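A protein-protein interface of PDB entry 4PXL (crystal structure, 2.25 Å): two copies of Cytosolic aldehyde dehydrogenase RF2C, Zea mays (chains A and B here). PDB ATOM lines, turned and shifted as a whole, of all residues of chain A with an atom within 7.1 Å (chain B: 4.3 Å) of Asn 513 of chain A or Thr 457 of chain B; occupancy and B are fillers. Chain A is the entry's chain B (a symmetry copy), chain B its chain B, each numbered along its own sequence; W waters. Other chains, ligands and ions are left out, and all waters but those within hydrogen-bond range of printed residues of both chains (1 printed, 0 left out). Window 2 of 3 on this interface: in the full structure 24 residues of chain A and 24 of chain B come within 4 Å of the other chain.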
ATOM      1  N   ARG A 165     -14.215  15.971   2.382  1.00  0.00           N
ATOM      2  CA  ARG A 165     -14.665  16.990   3.328  1.00  0.00           C
ATOM      3  C   ARG A 165     -15.927  16.445   4.009  1.00  0.00           C
ATOM      4  O   ARG A 165     -17.050  16.852   3.722  1.00  0.00           O
ATOM      5  CB  ARG A 165     -14.902  18.338   2.609  1.00  0.00           C
ATOM      6  CG  ARG A 165     -14.430  19.552   3.408  1.00  0.00           C
ATOM      7  CD  ARG A 165     -14.388  20.848   2.595  1.00  0.00           C
ATOM      8  NE  ARG A 165     -13.453  20.772   1.457  1.00  0.00           N
ATOM      9  CZ  ARG A 165     -13.155  21.781   0.640  1.00  0.00           C
ATOM     10  NH1 ARG A 165     -13.688  22.984   0.833  1.00  0.00           N
ATOM     11  NH2 ARG A 165     -12.308  21.600  -0.365  1.00  0.00           N
ATOM     12  N   LEU A 511     -18.927  18.072   5.594  1.00  0.00           N
ATOM     13  CA  LEU A 511     -18.505  19.235   6.415  1.00  0.00           C
ATOM     14  C   LEU A 511     -18.423  20.495   5.556  1.00  0.00           C
ATOM     15  O   LEU A 511     -18.048  20.414   4.392  1.00  0.00           O
ATOM     16  CB  LEU A 511     -17.137  19.025   7.075  1.00  0.00           C
ATOM     17  CG  LEU A 511     -17.074  17.982   8.158  1.00  0.00           C
ATOM     18  CD1 LEU A 511     -15.654  17.578   8.410  1.00  0.00           C
ATOM     19  CD2 LEU A 511     -17.908  18.378   9.399  1.00  0.00           C
ATOM     20  N   TYR A 512     -18.712  21.654   6.148  1.00  0.00           N
ATOM     21  CA  TYR A 512     -18.685  22.939   5.488  1.00  0.00           C
ATOM     22  C   TYR A 512     -17.800  23.891   6.277  1.00  0.00           C
ATOM     23  O   TYR A 512     -17.952  24.025   7.506  1.00  0.00           O
ATOM     24  CB  TYR A 512     -20.119  23.515   5.345  1.00  0.00           C
ATOM     25  CG  TYR A 512     -21.053  22.576   4.613  1.00  0.00           C
ATOM     26  CD1 TYR A 512     -21.070  22.520   3.220  1.00  0.00           C
ATOM     27  CD2 TYR A 512     -21.874  21.691   5.309  1.00  0.00           C
ATOM     28  CE1 TYR A 512     -21.855  21.588   2.543  1.00  0.00           C
ATOM     29  CE2 TYR A 512     -22.686  20.779   4.637  1.00  0.00           C
ATOM     30  CZ  TYR A 512     -22.684  20.742   3.255  1.00  0.00           C
ATOM     31  OH  TYR A 512     -23.523  19.876   2.591  1.00  0.00           O
ATOM     32  N   ASN A 513     -16.898  24.592   5.558  1.00  0.00           N
ATOM     33  CA  ASN A 513     -15.987  25.588   6.157  1.00  0.00           C
ATOM     34  C   ASN A 513     -15.224  25.057   7.363  1.00  0.00           C
ATOM     35  O   ASN A 513     -15.186  25.710   8.412  1.00  0.00           O
ATOM     36  CB  ASN A 513     -16.740  26.888   6.535  1.00  0.00           C
ATOM     37  CG  ASN A 513     -17.360  27.571   5.352  1.00  0.00           C
ATOM     38  OD1 ASN A 513     -16.690  27.875   4.355  1.00  0.00           O
ATOM     39  ND2 ASN A 513     -18.662  27.810   5.440  1.00  0.00           N
ATOM     40  N   THR A 514     -14.658  23.858   7.245  1.00  0.00           N
ATOM     41  CA  THR A 514     -13.900  23.338   8.380  1.00  0.00           C
ATOM     42  C   THR A 514     -12.471  23.935   8.390  1.00  0.00           C
ATOM     43  O   THR A 514     -11.843  23.995   7.329  1.00  0.00           O
ATOM     44  CB  THR A 514     -14.001  21.815   8.470  1.00  0.00           C
ATOM     45  OG1 THR A 514     -13.397  21.410   9.698  1.00  0.00           O
ATOM     46  CG2 THR A 514     -13.360  21.088   7.271  1.00  0.00           C
ATOM     47  N   PRO A 515     -11.975  24.446   9.547  1.00  0.00           N
ATOM     48  CA  PRO A 515     -10.603  24.992   9.587  1.00  0.00           C
ATOM     49  C   PRO A 515      -9.494  23.908   9.631  1.00  0.00           C
ATOM     50  O   PRO A 515      -8.308  24.218   9.553  1.00  0.00           O
ATOM     51  CB  PRO A 515     -10.611  25.869  10.846  1.00  0.00           C
ATOM     52  CG  PRO A 515     -11.582  25.173  11.763  1.00  0.00           C
ATOM     53  CD  PRO A 515     -12.621  24.497  10.875  1.00  0.00           C
ATOM     54  N   TRP A 516      -9.881  22.644   9.775  1.00  0.00           N
ATOM     55  CA  TRP A 516      -8.965  21.503   9.783  1.00  0.00           C
ATOM     56  C   TRP A 516      -9.725  20.271   9.306  1.00  0.00           C
ATOM     57  O   TRP A 516     -10.936  20.171   9.499  1.00  0.00           O
ATOM     58  CB  TRP A 516      -8.352  21.252  11.194  1.00  0.00           C
ATOM     59  CG  TRP A 516      -9.356  20.853  12.229  1.00  0.00           C
ATOM     60  CD1 TRP A 516     -10.096  21.684  13.019  1.00  0.00           C
ATOM     61  CD2 TRP A 516      -9.760  19.511  12.559  1.00  0.00           C
ATOM     62  NE1 TRP A 516     -10.911  20.946  13.843  1.00  0.00           N
ATOM     63  CE2 TRP A 516     -10.761  19.609  13.551  1.00  0.00           C
ATOM     64  CE3 TRP A 516      -9.396  18.240  12.084  1.00  0.00           C
ATOM     65  CZ2 TRP A 516     -11.366  18.483  14.121  1.00  0.00           C
ATOM     66  CZ3 TRP A 516     -10.013  17.128  12.631  1.00  0.00           C
ATOM     67  CH2 TRP A 516     -10.978  17.254  13.648  1.00  0.00           C
ATOM     68  N   ASP B 453     -25.258  21.350  10.295  1.00  0.00           N
ATOM     69  CA  ASP B 453     -24.107  21.975   9.633  1.00  0.00           C
ATOM     70  C   ASP B 453     -23.479  23.110  10.451  1.00  0.00           C
ATOM     71  O   ASP B 453     -22.254  23.149  10.607  1.00  0.00           O
ATOM     72  CB  ASP B 453     -24.473  22.436   8.193  1.00  0.00           C
ATOM     73  CG  ASP B 453     -24.852  21.270   7.288  1.00  0.00           C
ATOM     74  OD1 ASP B 453     -24.251  20.176   7.434  1.00  0.00           O
ATOM     75  OD2 ASP B 453     -25.748  21.441   6.447  1.00  0.00           O
ATOM     76  N   VAL B 454     -24.317  24.016  10.985  1.00  0.00           N
ATOM     77  CA  VAL B 454     -23.833  25.080  11.871  1.00  0.00           C
ATOM     78  C   VAL B 454     -23.148  24.433  13.088  1.00  0.00           C
ATOM     79  O   VAL B 454     -22.033  24.818  13.433  1.00  0.00           O
ATOM     80  CB  VAL B 454     -24.956  26.039  12.299  1.00  0.00           C
ATOM     81  CG1 VAL B 454     -24.450  27.061  13.315  1.00  0.00           C
ATOM     82  CG2 VAL B 454     -25.585  26.731  11.088  1.00  0.00           C
ATOM     83  N   ALA B 455     -23.803  23.437  13.711  1.00  0.00           N
ATOM     84  CA  ALA B 455     -23.262  22.745  14.889  1.00  0.00           C
ATOM     85  C   ALA B 455     -21.894  22.122  14.587  1.00  0.00           C
ATOM     86  O   ALA B 455     -20.953  22.340  15.351  1.00  0.00           O
ATOM     87  CB  ALA B 455     -24.243  21.682  15.376  1.00  0.00           C
ATOM     88  N   ASN B 456     -21.764  21.424  13.443  1.00  0.00           N
ATOM     89  CA  ASN B 456     -20.475  20.823  13.051  1.00  0.00           C
ATOM     90  C   ASN B 456     -19.398  21.843  12.728  1.00  0.00           C
ATOM     91  O   ASN B 456     -18.278  21.662  13.174  1.00  0.00           O
ATOM     92  CB  ASN B 456     -20.630  19.836  11.900  1.00  0.00           C
ATOM     93  CG  ASN B 456     -21.262  18.526  12.303  1.00  0.00           C
ATOM     94  OD1 ASN B 456     -21.264  18.142  13.470  1.00  0.00           O
ATOM     95  ND2 ASN B 456     -21.806  17.793  11.345  1.00  0.00           N
ATOM     96  N   THR B 457     -19.726  22.902  11.967  1.00  0.00           N
ATOM     97  CA  THR B 457     -18.757  23.959  11.614  1.00  0.00           C
ATOM     98  C   THR B 457     -18.262  24.683  12.870  1.00  0.00           C
ATOM     99  O   THR B 457     -17.063  24.819  13.059  1.00  0.00           O
ATOM    100  CB  THR B 457     -19.363  24.943  10.573  1.00  0.00           C
ATOM    101  OG1 THR B 457     -19.740  24.217   9.415  1.00  0.00           O
ATOM    102  CG2 THR B 457     -18.392  26.067  10.168  1.00  0.00           C
ATOM    103  N   VAL B 458     -19.187  25.124  13.731  1.00  0.00           N
ATOM    104  CA  VAL B 458     -18.871  25.866  14.956  1.00  0.00           C
ATOM    105  C   VAL B 458     -18.086  25.027  15.962  1.00  0.00           C
ATOM    106  O   VAL B 458     -17.062  25.508  16.445  1.00  0.00           O
ATOM    107  CB  VAL B 458     -20.116  26.590  15.533  1.00  0.00           C
ATOM    108  CG1 VAL B 458     -19.794  27.347  16.825  1.00  0.00           C
ATOM    109  CG2 VAL B 458     -20.697  27.536  14.497  1.00  0.00           C
ATOM    110  N   SER B 459     -18.514  23.766  16.229  1.00  0.00           N
ATOM    111  CA  SER B 459     -17.822  22.869  17.190  1.00  0.00           C
ATOM    112  C   SER B 459     -16.371  22.566  16.793  1.00  0.00           C
ATOM    113  O   SER B 459     -15.487  22.510  17.654  1.00  0.00           O
ATOM    114  CB  SER B 459     -18.597  21.567  17.405  1.00  0.00           C
ATOM    115  OG  SER B 459     -18.778  20.841  16.197  1.00  0.00           O
ATOM    116  N   ARG B 460     -16.126  22.392  15.500  1.00  0.00           N
ATOM    117  CA  ARG B 460     -14.783  22.099  15.023  1.00  0.00           C
ATOM    118  C   ARG B 460     -13.872  23.337  15.010  1.00  0.00           C
ATOM    119  O   ARG B 460     -12.651  23.204  15.003  1.00  0.00           O
ATOM    120  CB  ARG B 460     -14.866  21.518  13.620  1.00  0.00           C
ATOM    121  CG  ARG B 460     -15.394  20.066  13.593  1.00  0.00           C
ATOM    122  CD  ARG B 460     -15.687  19.705  12.155  1.00  0.00           C
ATOM    123  NE  ARG B 460     -14.441  19.415  11.430  1.00  0.00           N
ATOM    124  CZ  ARG B 460     -13.874  18.217  11.403  1.00  0.00           C
ATOM    125  NH1 ARG B 460     -14.438  17.197  12.030  1.00  0.00           N
ATOM    126  NH2 ARG B 460     -12.771  18.019  10.706  1.00  0.00           N
ATOM    127  N   SER B 461     -14.467  24.532  14.973  1.00  0.00           N
ATOM    128  CA  SER B 461     -13.776  25.820  14.868  1.00  0.00           C
ATOM    129  C   SER B 461     -13.462  26.511  16.204  1.00  0.00           C
ATOM    130  O   SER B 461     -12.591  27.393  16.256  1.00  0.00           O
ATOM    131  CB  SER B 461     -14.574  26.749  13.971  1.00  0.00           C
ATOM    132  OG  SER B 461     -14.814  26.128  12.717  1.00  0.00           O
HETATM  133  O   HOH W   1     -25.452  19.234   4.477  1.00  0.00           O
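CD2 of Leu 511 of chain A touches CB of Asn 456 of chain B, 3.97 Å away. CD1 of Leu 511 of chain A touches CZ of Arg 460 of chain B, at 3.5 Å. Tyr 512 of chain A touches Asp 453 of chain B (CE2 to OD1, 3.3 Å). Asn 513 of chain A touches Thr 457 of chain B. Arg 460 of chain B touches Pro 515 of chain A (O to CG, 3.9 Å). Ser 461 of chain B touches Pro 515 of chain A (OG to CD, 3.3 Å).
Among the printed residues, no Asp or Glu carboxylate lies within 4 Å of a Lys or Arg side-chain nitrogen of the other chain.
Water W1 lies within hydrogen-bond range of OH of Tyr 512 of chain A (2.8 Å) and OD2 of Asp 453 of chain B (3.0 Å).
Arg 165 of chain A touches none of the printed residues of chain B. Of the printed residues of chain B, Tyr 512 of chain A touches Asp 453 (3.3 Å) and Thr 457 (2.6 Å). Of the printed residues of chain B, Asn 513 of chain A touches Thr 457 (3.7 Å). Of the printed residues of chain B, Pro 515 of chain A touches Arg 460 and Ser 461. Printed residues of chain A within 4 Å of Asp 453 of chain B: Tyr 512. Thr 457 of chain B touches two residues of chain A. Of the printed residues of chain A, Ser 461 of chain B touches Pro 515 (3.3 Å). The nearest residue of chain A that does not touch Thr 457 of chain B is Pro 515 of chain A (5.0 Å). The nearest printed residue of chain A that does not touch Ser 461 of chain B is Asn 513 of chain A (4.3 Å).
The side-chain hydroxyl of Ser 461 of chain B is in hydrogen-bond range of the backbone carbonyl oxygen of Thr 457 of chain B, 2.6 Å away. The backbone carbonyl oxygen (O) of Asn 456 of chain B is in hydrogen-bond range of the side-chain hydroxyl (OG) of Ser 459 of chain B. O of Trp 516 of chain A lies within hydrogen-bond range of OG1 of Thr 514 of chain A, 2.8 Å away. The backbone carbonyl oxygen (O) of Arg 165 of chain A lies within hydrogen-bond range of the backbone NH (N) of Leu 511 of chain A (2.9 Å). The backbone carbonyl oxygen of Asp 453 of chain B sits at hydrogen-bond distance from the side-chain hydroxyl of Thr 457 of chain B (3.0 Å).
No position is printed for both chains.
The guanidinium group (NE) of Arg 460 of chain B sits at hydrogen-bond distance from the side-chain hydroxyl (OG1) of Thr 514 of chain A, at 2.8 Å. The side-chain hydroxyl (OG1) of Thr 457 of chain B sits at hydrogen-bond distance from the backbone carbonyl oxygen (O) of Tyr 512 of chain A, at 2.6 Å. The guanidinium group (NH2) of Arg 460 of chain B lies within hydrogen-bond range of the backbone carbonyl oxygen (O) of Trp 516 of chain A, at 3.1 Å.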
